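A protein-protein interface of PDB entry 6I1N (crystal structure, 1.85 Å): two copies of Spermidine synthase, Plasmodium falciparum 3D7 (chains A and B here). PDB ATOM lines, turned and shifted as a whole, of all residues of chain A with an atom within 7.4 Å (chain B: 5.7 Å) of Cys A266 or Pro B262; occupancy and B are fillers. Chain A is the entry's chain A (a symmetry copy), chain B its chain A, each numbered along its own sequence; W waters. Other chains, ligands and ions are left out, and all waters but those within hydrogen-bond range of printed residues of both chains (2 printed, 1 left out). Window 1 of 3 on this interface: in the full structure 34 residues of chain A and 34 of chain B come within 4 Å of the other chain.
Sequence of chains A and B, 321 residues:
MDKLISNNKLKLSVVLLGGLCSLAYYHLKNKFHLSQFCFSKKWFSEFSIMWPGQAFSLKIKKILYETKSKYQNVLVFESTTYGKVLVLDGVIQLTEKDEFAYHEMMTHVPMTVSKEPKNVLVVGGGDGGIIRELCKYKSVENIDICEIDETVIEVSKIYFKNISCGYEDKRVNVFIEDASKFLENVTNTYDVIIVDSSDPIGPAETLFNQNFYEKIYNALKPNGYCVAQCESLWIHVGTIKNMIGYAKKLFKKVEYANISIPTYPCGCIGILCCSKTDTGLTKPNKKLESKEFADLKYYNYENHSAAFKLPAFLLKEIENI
OE1 of Gln A54 is in hydrogen-bond range of OH of Tyr B82 (2.8 Å).
NE1 of Trp A234 sits at hydrogen-bond distance from OG of Ser B260 (3.1 Å).
The side-chain hydroxyl (OH) of Tyr B82 is in hydrogen-bond range of the side-chain sulfur (SG) of Cys A266 (3.3 Å).
The side-chain sulfur of Cys A266 sits at hydrogen-bond distance from the side-chain amide nitrogen of Gln A54 (3.5 Å).
The side-chain carboxylate (OD2) of Asp B98 sits at hydrogen-bond distance from the side-chain hydroxyl (OG1) of Thr B263.
The backbone NH (N) of Trp A234 lies close to the side-chain hydroxyl (OG) of Ser A232 (3.4 Å).
Among the printed residues, merely in contact across the chains: Trp A234 with Asp B98 (3.6 Å), Trp A234 with Pro B262 (3.4 Å) and Cys A266 with Pro B262 (3.6 Å).
Pro B262 touches just these residues of chain A: Trp A234 and Cys A266.
Printed residues of chain A within 4 Å of Ser B260: Trp A234.
Printed residues of chain A within 4 Å of Asp B98: Trp A234 (3.6 Å).
Of the printed residues of chain A, Tyr B82 touches Gln A54 (2.8 Å) and Cys A266 (3.3 Å).
Printed residues of chain B within 4 Å of Trp A234: Asp B98 (3.6 Å), Ser B260 (3.1 Å) and Pro B262 (3.4 Å).
Printed residues of chain B within 4 Å of Gln A54: Tyr B82 (2.8 Å).
Ile A269 touches none of the printed residues of chain B.
The nearest residue of chain A that does not touch Pro B262 is Gly A267 (5.4 Å).
The nearest printed residue of chain A that does not touch Tyr B82 is Ile A235 (4.2 Å).
Of the 19 printed residues of chain A, 3 touch a printed residue of chain B.
Hydrophobic or aromatic side chains of chain B that line the printed part of chain A: Tyr B82 and Pro B262.
Among the printed residues, 6 pairs touch across the chains.
Among the printed residues, no Asp or Glu carboxylate lies within 4 Å of a Lys or Arg side-chain nitrogen of the other chain.
Positions printed for both chains: 56, 261, 262, 263, 264, 265, 267 and 268.
Water W1 lies within hydrogen-bond range of the backbone carbonyl oxygen of Gly A267 (2.8 Å), the backbone carbonyl oxygen of Gly B267 (3.5 Å) and the side-chain sulfur of Cys B268 (3.7 Å).
Water W2 lies within hydrogen-bond range of O of Gly B267 (3.5 Å), O of Gly A267 (3.5 Å) and OG of Ser B260 (3.5 Å).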
ATOM      1  N   GLU A  46      12.696  -1.870  -5.953  1.00  0.00           N
ATOM      2  CA  GLU A  46      12.745  -0.651  -6.751  1.00  0.00           C
ATOM      3  C   GLU A  46      11.617  -0.701  -7.781  1.00  0.00           C
ATOM      4  O   GLU A  46      11.742  -1.353  -8.823  1.00  0.00           O
ATOM      5  CB  GLU A  46      14.110  -0.529  -7.426  1.00  0.00           C
ATOM      6  CG  GLU A  46      14.263   0.719  -8.256  1.00  0.00           C
ATOM      7  CD  GLU A  46      15.552   0.747  -9.017  1.00  0.00           C
ATOM      8  OE1 GLU A  46      15.830  -0.237  -9.734  1.00  0.00           O
ATOM      9  OE2 GLU A  46      16.285   1.751  -8.921  1.00  0.00           O
ATOM     10  N   TRP A  51       9.675   2.408 -15.308  1.00  0.00           N
ATOM     11  CA  TRP A  51       9.854   1.050 -15.824  1.00  0.00           C
ATOM     12  C   TRP A  51       8.715   0.195 -15.287  1.00  0.00           C
ATOM     13  O   TRP A  51       8.910  -0.640 -14.390  1.00  0.00           O
ATOM     14  CB  TRP A  51      11.221   0.463 -15.462  1.00  0.00           C
ATOM     15  CG  TRP A  51      11.739   0.788 -14.088  1.00  0.00           C
ATOM     16  CD1 TRP A  51      11.617   0.024 -12.951  1.00  0.00           C
ATOM     17  CD2 TRP A  51      12.504   1.939 -13.712  1.00  0.00           C
ATOM     18  NE1 TRP A  51      12.247   0.640 -11.893  1.00  0.00           N
ATOM     19  CE2 TRP A  51      12.806   1.812 -12.337  1.00  0.00           C
ATOM     20  CE3 TRP A  51      12.958   3.066 -14.402  1.00  0.00           C
ATOM     21  CZ2 TRP A  51      13.532   2.776 -11.641  1.00  0.00           C
ATOM     22  CZ3 TRP A  51      13.678   4.026 -13.708  1.00  0.00           C
ATOM     23  CH2 TRP A  51      13.962   3.874 -12.346  1.00  0.00           C
ATOM     24  N   GLN A  54       8.162  -4.135 -14.046  1.00  0.00           N
ATOM     25  CA  GLN A  54       9.382  -4.801 -13.616  1.00  0.00           C
ATOM     26  C   GLN A  54       9.853  -4.179 -12.318  1.00  0.00           C
ATOM     27  O   GLN A  54       9.465  -3.064 -11.969  1.00  0.00           O
ATOM     28  CB  GLN A  54      10.496  -4.701 -14.683  1.00  0.00           C
ATOM     29  CG  GLN A  54      11.038  -3.296 -14.824  1.00  0.00           C
ATOM     30  CD  GLN A  54      11.995  -3.159 -15.989  1.00  0.00           C
ATOM     31  OE1 GLN A  54      11.578  -3.028 -17.143  1.00  0.00           O
ATOM     32  NE2 GLN A  54      13.292  -3.208 -15.697  1.00  0.00           N
ATOM     33  N   PHE A  56      13.548  -4.497  -9.498  1.00  0.00           N
ATOM     34  CA  PHE A  56      14.764  -5.114  -8.986  1.00  0.00           C
ATOM     35  C   PHE A  56      14.786  -5.008  -7.459  1.00  0.00           C
ATOM     36  O   PHE A  56      14.359  -3.996  -6.900  1.00  0.00           O
ATOM     37  CB  PHE A  56      16.007  -4.420  -9.604  1.00  0.00           C
ATOM     38  CG  PHE A  56      17.299  -5.035  -9.204  1.00  0.00           C
ATOM     39  CD1 PHE A  56      17.629  -6.318  -9.605  1.00  0.00           C
ATOM     40  CD2 PHE A  56      18.229  -4.307  -8.448  1.00  0.00           C
ATOM     41  CE1 PHE A  56      18.842  -6.903  -9.208  1.00  0.00           C
ATOM     42  CE2 PHE A  56      19.437  -4.862  -8.075  1.00  0.00           C
ATOM     43  CZ  PHE A  56      19.754  -6.158  -8.449  1.00  0.00           C
ATOM     44  N   SER A 232      18.010   3.639 -20.396  1.00  0.00           N
ATOM     45  CA  SER A 232      18.339   2.305 -20.878  1.00  0.00           C
ATOM     46  C   SER A 232      17.722   2.095 -22.259  1.00  0.00           C
ATOM     47  O   SER A 232      16.559   2.431 -22.483  1.00  0.00           O
ATOM     48  CB  SER A 232      17.811   1.256 -19.902  1.00  0.00           C
ATOM     49  OG  SER A 232      18.129  -0.035 -20.341  1.00  0.00           O
ATOM     50  N   LEU A 233      18.500   1.538 -23.182  1.00  0.00           N
ATOM     51  CA  LEU A 233      17.996   1.260 -24.524  1.00  0.00           C
ATOM     52  C   LEU A 233      16.922   0.175 -24.531  1.00  0.00           C
ATOM     53  O   LEU A 233      16.201   0.042 -25.526  1.00  0.00           O
ATOM     54  CB  LEU A 233      19.137   0.848 -25.445  1.00  0.00           C
ATOM     55  CG  LEU A 233      20.071  -0.284 -24.990  1.00  0.00           C
ATOM     56  CD1 LEU A 233      19.537  -1.665 -25.408  1.00  0.00           C
ATOM     57  CD2 LEU A 233      21.408  -0.076 -25.638  1.00  0.00           C
ATOM     58  N   TRP A 234      16.800  -0.578 -23.451  1.00  0.00           N
ATOM     59  CA  TRP A 234      15.750  -1.586 -23.329  1.00  0.00           C
ATOM     60  C   TRP A 234      14.381  -1.029 -22.942  1.00  0.00           C
ATOM     61  O   TRP A 234      13.400  -1.779 -23.020  1.00  0.00           O
ATOM     62  CB  TRP A 234      16.186  -2.641 -22.312  1.00  0.00           C
ATOM     63  CG  TRP A 234      17.228  -3.543 -22.880  1.00  0.00           C
ATOM     64  CD1 TRP A 234      18.557  -3.587 -22.545  1.00  0.00           C
ATOM     65  CD2 TRP A 234      17.038  -4.522 -23.917  1.00  0.00           C
ATOM     66  NE1 TRP A 234      19.196  -4.556 -23.302  1.00  0.00           N
ATOM     67  CE2 TRP A 234      18.293  -5.129 -24.155  1.00  0.00           C
ATOM     68  CE3 TRP A 234      15.928  -4.946 -24.659  1.00  0.00           C
ATOM     69  CZ2 TRP A 234      18.477  -6.147 -25.114  1.00  0.00           C
ATOM     70  CZ3 TRP A 234      16.106  -5.969 -25.616  1.00  0.00           C
ATOM     71  CH2 TRP A 234      17.373  -6.551 -25.830  1.00  0.00           C
ATOM     72  N   ILE A 235      14.258   0.234 -22.519  1.00  0.00           N
ATOM     73  CA  ILE A 235      12.936   0.670 -22.064  1.00  0.00           C
ATOM     74  C   ILE A 235      12.485   2.025 -22.586  1.00  0.00           C
ATOM     75  O   ILE A 235      11.286   2.238 -22.777  1.00  0.00           O
ATOM     76  CB  ILE A 235      12.824   0.654 -20.524  1.00  0.00           C
ATOM     77  CG1 ILE A 235      14.072   1.221 -19.880  1.00  0.00           C
ATOM     78  CG2 ILE A 235      12.499  -0.764 -20.027  1.00  0.00           C
ATOM     79  CD1 ILE A 235      14.120   1.064 -18.375  1.00  0.00           C
ATOM     80  N   HIS A 236      13.390   2.963 -22.811  1.00  0.00           N
ATOM     81  CA  HIS A 236      12.961   4.300 -23.225  1.00  0.00           C
ATOM     82  C   HIS A 236      13.650   4.736 -24.527  1.00  0.00           C
ATOM     83  O   HIS A 236      14.349   5.750 -24.568  1.00  0.00           O
ATOM     84  CB  HIS A 236      13.178   5.295 -22.088  1.00  0.00           C
ATOM     85  CG  HIS A 236      12.101   5.230 -21.053  1.00  0.00           C
ATOM     86  ND1 HIS A 236      10.792   5.570 -21.330  1.00  0.00           N
ATOM     87  CD2 HIS A 236      12.123   4.838 -19.757  1.00  0.00           C
ATOM     88  CE1 HIS A 236      10.056   5.403 -20.244  1.00  0.00           C
ATOM     89  NE2 HIS A 236      10.840   4.963 -19.274  1.00  0.00           N
ATOM     90  N   ILE A 259      26.497   1.396 -21.094  1.00  0.00           N
ATOM     91  CA  ILE A 259      27.284   0.921 -19.957  1.00  0.00           C
ATOM     92  C   ILE A 259      26.557  -0.250 -19.315  1.00  0.00           C
ATOM     93  O   ILE A 259      25.368  -0.150 -19.022  1.00  0.00           O
ATOM     94  CB  ILE A 259      27.465   2.016 -18.886  1.00  0.00           C
ATOM     95  CG1 ILE A 259      28.095   3.289 -19.471  1.00  0.00           C
ATOM     96  CG2 ILE A 259      28.267   1.469 -17.714  1.00  0.00           C
ATOM     97  CD1 ILE A 259      27.987   4.492 -18.482  1.00  0.00           C
ATOM     98  N   ILE A 261      25.648  -2.134 -16.139  1.00  0.00           N
ATOM     99  CA  ILE A 261      25.687  -1.951 -14.696  1.00  0.00           C
ATOM    100  C   ILE A 261      24.430  -2.580 -14.099  1.00  0.00           C
ATOM    101  O   ILE A 261      23.300  -2.182 -14.437  1.00  0.00           O
ATOM    102  CB  ILE A 261      25.876  -0.469 -14.307  1.00  0.00           C
ATOM    103  CG1 ILE A 261      25.620  -0.259 -12.804  1.00  0.00           C
ATOM    104  CG2 ILE A 261      25.012   0.468 -15.134  1.00  0.00           C
ATOM    105  CD1 ILE A 261      26.370   0.997 -12.235  1.00  0.00           C
ATOM    106  N   PRO A 262      24.592  -3.580 -13.228  1.00  0.00           N
ATOM    107  CA  PRO A 262      23.450  -4.454 -12.904  1.00  0.00           C
ATOM    108  C   PRO A 262      22.401  -3.803 -12.014  1.00  0.00           C
ATOM    109  O   PRO A 262      21.238  -4.226 -12.052  1.00  0.00           O
ATOM    110  CB  PRO A 262      24.116  -5.659 -12.212  1.00  0.00           C
ATOM    111  CG  PRO A 262      25.409  -5.158 -11.736  1.00  0.00           C
ATOM    112  CD  PRO A 262      25.857  -4.130 -12.719  1.00  0.00           C
ATOM    113  N   THR A 263      22.744  -2.783 -11.239  1.00  0.00           N
ATOM    114  CA  THR A 263      21.754  -2.224 -10.334  1.00  0.00           C
ATOM    115  C   THR A 263      21.051  -1.025 -10.933  1.00  0.00           C
ATOM    116  O   THR A 263      20.312  -0.336 -10.229  1.00  0.00           O
ATOM    117  CB  THR A 263      22.386  -1.864  -8.984  1.00  0.00           C
ATOM    118  OG1 THR A 263      23.447  -0.918  -9.167  1.00  0.00           O
ATOM    119  CG2 THR A 263      22.951  -3.118  -8.287  1.00  0.00           C
ATOM    120  N   TYR A 264      21.286  -0.744 -12.206  1.00  0.00           N
ATOM    121  CA  TYR A 264      20.355   0.171 -12.838  1.00  0.00           C
ATOM    122  C   TYR A 264      19.293  -0.630 -13.589  1.00  0.00           C
ATOM    123  O   TYR A 264      19.563  -1.759 -13.999  1.00  0.00           O
ATOM    124  CB  TYR A 264      21.087   1.105 -13.800  1.00  0.00           C
ATOM    125  CG  TYR A 264      21.815   2.221 -13.065  1.00  0.00           C
ATOM    126  CD1 TYR A 264      21.447   2.606 -11.763  1.00  0.00           C
ATOM    127  CD2 TYR A 264      22.849   2.860 -13.635  1.00  0.00           C
ATOM    128  CE1 TYR A 264      22.133   3.639 -11.096  1.00  0.00           C
ATOM    129  CE2 TYR A 264      23.530   3.877 -12.988  1.00  0.00           C
ATOM    130  CZ  TYR A 264      23.186   4.274 -11.750  1.00  0.00           C
ATOM    131  OH  TYR A 264      23.926   5.302 -11.177  1.00  0.00           O
ATOM    132  N   PRO A 265      18.096  -0.067 -13.768  1.00  0.00           N
ATOM    133  CA  PRO A 265      17.000  -0.812 -14.418  1.00  0.00           C
ATOM    134  C   PRO A 265      17.431  -1.370 -15.763  1.00  0.00           C
ATOM    135  O   PRO A 265      18.011  -0.661 -16.592  1.00  0.00           O
ATOM    136  CB  PRO A 265      15.904   0.242 -14.587  1.00  0.00           C
ATOM    137  CG  PRO A 265      16.172   1.246 -13.490  1.00  0.00           C
ATOM    138  CD  PRO A 265      17.687   1.295 -13.377  1.00  0.00           C
ATOM    139  N   CYS A 266      17.155  -2.657 -15.971  1.00  0.00           N
ATOM    140  CA  CYS A 266      17.472  -3.386 -17.206  1.00  0.00           C
ATOM    141  C   CYS A 266      18.961  -3.683 -17.316  1.00  0.00           C
ATOM    142  O   CYS A 266      19.413  -4.223 -18.349  1.00  0.00           O
ATOM    143  CB  CYS A 266      16.972  -2.650 -18.460  1.00  0.00           C
ATOM    144  SG  CYS A 266      15.134  -2.638 -18.616  1.00  0.00           S
ATOM    145  N   GLY A 267      19.747  -3.324 -16.288  1.00  0.00           N
ATOM    146  CA  GLY A 267      21.132  -3.726 -16.225  1.00  0.00           C
ATOM    147  C   GLY A 267      22.058  -2.887 -17.059  1.00  0.00           C
ATOM    148  O   GLY A 267      23.215  -3.271 -17.243  1.00  0.00           O
ATOM    149  N   CYS A 268      21.595  -1.753 -17.568  1.00  0.00           N
ATOM    150  CA  CYS A 268      22.470  -0.910 -18.370  1.00  0.00           C
ATOM    151  C   CYS A 268      21.918   0.510 -18.382  1.00  0.00           C
ATOM    152  O   CYS A 268      20.782   0.756 -17.983  1.00  0.00           O
ATOM    153  CB  CYS A 268      22.606  -1.475 -19.792  1.00  0.00           C
ATOM    154  SG  CYS A 268      21.095  -1.454 -20.767  1.00  0.00           S
ATOM    155  N   ILE A 269      22.748   1.451 -18.846  1.00  0.00           N
ATOM    156  CA  ILE A 269      22.377   2.862 -18.885  1.00  0.00           C
ATOM    157  C   ILE A 269      23.213   3.532 -19.967  1.00  0.00           C
ATOM    158  O   ILE A 269      24.390   3.218 -20.122  1.00  0.00           O
ATOM    159  CB  ILE A 269      22.585   3.547 -17.501  1.00  0.00           C
ATOM    160  CG1 ILE A 269      22.016   4.952 -17.513  1.00  0.00           C
ATOM    161  CG2 ILE A 269      24.076   3.650 -17.105  1.00  0.00           C
ATOM    162  CD1 ILE A 269      20.541   4.978 -17.656  1.00  0.00           C
ATOM    163  N   PHE B  56      14.941 -10.345  -9.480  1.00  0.00           N
ATOM    164  CA  PHE B  56      14.233  -9.609 -10.519  1.00  0.00           C
ATOM    165  C   PHE B  56      12.768 -10.054 -10.551  1.00  0.00           C
ATOM    166  O   PHE B  56      12.473 -11.236 -10.362  1.00  0.00           O
ATOM    167  CB  PHE B  56      14.913  -9.852 -11.892  1.00  0.00           C
ATOM    168  CG  PHE B  56      14.309  -9.075 -13.006  1.00  0.00           C
ATOM    169  CD1 PHE B  56      14.397  -7.693 -13.037  1.00  0.00           C
ATOM    170  CD2 PHE B  56      13.677  -9.733 -14.071  1.00  0.00           C
ATOM    171  CE1 PHE B  56      13.807  -6.963 -14.081  1.00  0.00           C
ATOM    172  CE2 PHE B  56      13.119  -9.024 -15.117  1.00  0.00           C
ATOM    173  CZ  PHE B  56      13.178  -7.640 -15.132  1.00  0.00           C
ATOM    174  N   TYR B  82       6.752  -7.392 -20.852  1.00  0.00           N
ATOM    175  CA  TYR B  82       7.779  -8.148 -21.562  1.00  0.00           C
ATOM    176  C   TYR B  82       7.183  -9.249 -22.445  1.00  0.00           C
ATOM    177  O   TYR B  82       7.908 -10.152 -22.899  1.00  0.00           O
ATOM    178  CB  TYR B  82       8.793  -8.721 -20.560  1.00  0.00           C
ATOM    179  CG  TYR B  82       9.825  -7.685 -20.109  1.00  0.00           C
ATOM    180  CD1 TYR B  82       9.470  -6.647 -19.261  1.00  0.00           C
ATOM    181  CD2 TYR B  82      11.133  -7.726 -20.580  1.00  0.00           C
ATOM    182  CE1 TYR B  82      10.417  -5.681 -18.872  1.00  0.00           C
ATOM    183  CE2 TYR B  82      12.079  -6.775 -20.198  1.00  0.00           C
ATOM    184  CZ  TYR B  82      11.719  -5.764 -19.348  1.00  0.00           C
ATOM    185  OH  TYR B  82      12.668  -4.819 -18.992  1.00  0.00           O
ATOM    186  N   ASP B  98      12.915  -9.611 -25.207  1.00  0.00           N
ATOM    187  CA  ASP B  98      14.358  -9.512 -25.377  1.00  0.00           C
ATOM    188  C   ASP B  98      15.068 -10.791 -25.819  1.00  0.00           C
ATOM    189  O   ASP B  98      16.302 -10.789 -25.879  1.00  0.00           O
ATOM    190  CB  ASP B  98      15.018  -9.033 -24.067  1.00  0.00           C
ATOM    191  CG  ASP B  98      14.807 -10.014 -22.917  1.00  0.00           C
ATOM    192  OD1 ASP B  98      14.160 -11.095 -23.128  1.00  0.00           O
ATOM    193  OD2 ASP B  98      15.257  -9.697 -21.794  1.00  0.00           O
ATOM    194  N   SER B 260      24.075  -8.157 -23.654  1.00  0.00           N
ATOM    195  CA  SER B 260      23.187  -7.385 -22.809  1.00  0.00           C
ATOM    196  C   SER B 260      21.782  -7.948 -22.962  1.00  0.00           C
ATOM    197  O   SER B 260      21.237  -7.969 -24.071  1.00  0.00           O
ATOM    198  CB  SER B 260      23.231  -5.905 -23.187  1.00  0.00           C
ATOM    199  OG  SER B 260      22.123  -5.211 -22.657  1.00  0.00           O
ATOM    200  N   ILE B 261      21.196  -8.396 -21.856  1.00  0.00           N
ATOM    201  CA  ILE B 261      19.829  -8.891 -21.923  1.00  0.00           C
ATOM    202  C   ILE B 261      19.185  -8.708 -20.551  1.00  0.00           C
ATOM    203  O   ILE B 261      19.670  -9.259 -19.545  1.00  0.00           O
ATOM    204  CB  ILE B 261      19.766 -10.344 -22.443  1.00  0.00           C
ATOM    205  CG1 ILE B 261      18.366 -10.943 -22.228  1.00  0.00           C
ATOM    206  CG2 ILE B 261      20.830 -11.234 -21.823  1.00  0.00           C
ATOM    207  CD1 ILE B 261      18.043 -12.098 -23.242  1.00  0.00           C
ATOM    208  N   PRO B 262      18.107  -7.924 -20.472  1.00  0.00           N
ATOM    209  CA  PRO B 262      17.667  -7.422 -19.158  1.00  0.00           C
ATOM    210  C   PRO B 262      17.008  -8.473 -18.278  1.00  0.00           C
ATOM    211  O   PRO B 262      17.022  -8.321 -17.050  1.00  0.00           O
ATOM    212  CB  PRO B 262      16.687  -6.290 -19.525  1.00  0.00           C
ATOM    213  CG  PRO B 262      16.257  -6.589 -20.893  1.00  0.00           C
ATOM    214  CD  PRO B 262      17.414  -7.239 -21.573  1.00  0.00           C
ATOM    215  N   THR B 263      16.458  -9.543 -18.839  1.00  0.00           N
ATOM    216  CA  THR B 263      15.760 -10.498 -17.995  1.00  0.00           C
ATOM    217  C   THR B 263      16.650 -11.653 -17.590  1.00  0.00           C
ATOM    218  O   THR B 263      16.162 -12.630 -17.022  1.00  0.00           O
ATOM    219  CB  THR B 263      14.488 -11.008 -18.682  1.00  0.00           C
ATOM    220  OG1 THR B 263      14.810 -11.629 -19.932  1.00  0.00           O
ATOM    221  CG2 THR B 263      13.498  -9.854 -18.939  1.00  0.00           C
ATOM    222  N   TYR B 264      17.937 -11.577 -17.895  1.00  0.00           N
ATOM    223  CA  TYR B 264      18.812 -12.506 -17.202  1.00  0.00           C
ATOM    224  C   TYR B 264      19.429 -11.809 -15.992  1.00  0.00           C
ATOM    225  O   TYR B 264      19.563 -10.585 -16.000  1.00  0.00           O
ATOM    226  CB  TYR B 264      19.910 -13.009 -18.136  1.00  0.00           C
ATOM    227  CG  TYR B 264      19.397 -14.075 -19.094  1.00  0.00           C
ATOM    228  CD1 TYR B 264      18.236 -14.818 -18.813  1.00  0.00           C
ATOM    229  CD2 TYR B 264      20.029 -14.323 -20.252  1.00  0.00           C
ATOM    230  CE1 TYR B 264      17.774 -15.799 -19.711  1.00  0.00           C
ATOM    231  CE2 TYR B 264      19.583 -15.284 -21.142  1.00  0.00           C
ATOM    232  CZ  TYR B 264      18.487 -16.018 -20.888  1.00  0.00           C
ATOM    233  OH  TYR B 264      18.112 -16.961 -21.837  1.00  0.00           O
ATOM    234  N   PRO B 265      19.801 -12.565 -14.957  1.00  0.00           N
ATOM    235  CA  PRO B 265      20.335 -11.952 -13.725  1.00  0.00           C
ATOM    236  C   PRO B 265      21.496 -11.020 -14.028  1.00  0.00           C
ATOM    237  O   PRO B 265      22.423 -11.376 -14.763  1.00  0.00           O
ATOM    238  CB  PRO B 265      20.799 -13.155 -12.901  1.00  0.00           C
ATOM    239  CG  PRO B 265      19.937 -14.299 -13.381  1.00  0.00           C
ATOM    240  CD  PRO B 265      19.745 -14.036 -14.867  1.00  0.00           C
ATOM    241  N   GLY B 267      21.435  -8.536 -15.840  1.00  0.00           N
ATOM    242  CA  GLY B 267      21.201  -7.865 -17.097  1.00  0.00           C
ATOM    243  C   GLY B 267      22.142  -8.264 -18.197  1.00  0.00           C
ATOM    244  O   GLY B 267      22.167  -7.603 -19.237  1.00  0.00           O
ATOM    245  N   CYS B 268      22.916  -9.326 -18.010  1.00  0.00           N
ATOM    246  CA  CYS B 268      23.830  -9.749 -19.062  1.00  0.00           C
ATOM    247  C   CYS B 268      24.188 -11.213 -18.849  1.00  0.00           C
ATOM    248  O   CYS B 268      23.922 -11.789 -17.796  1.00  0.00           O
ATOM    249  CB  CYS B 268      25.081  -8.857 -19.077  1.00  0.00           C
ATOM    250  SG  CYS B 268      26.127  -8.987 -17.619  1.00  0.00           S
HETATM  251  O   HOH W   1      24.458  -5.720 -17.393  1.00  0.00           O
HETATM  252  O   HOH W   2      24.383  -5.040 -19.992  1.00  0.00           O
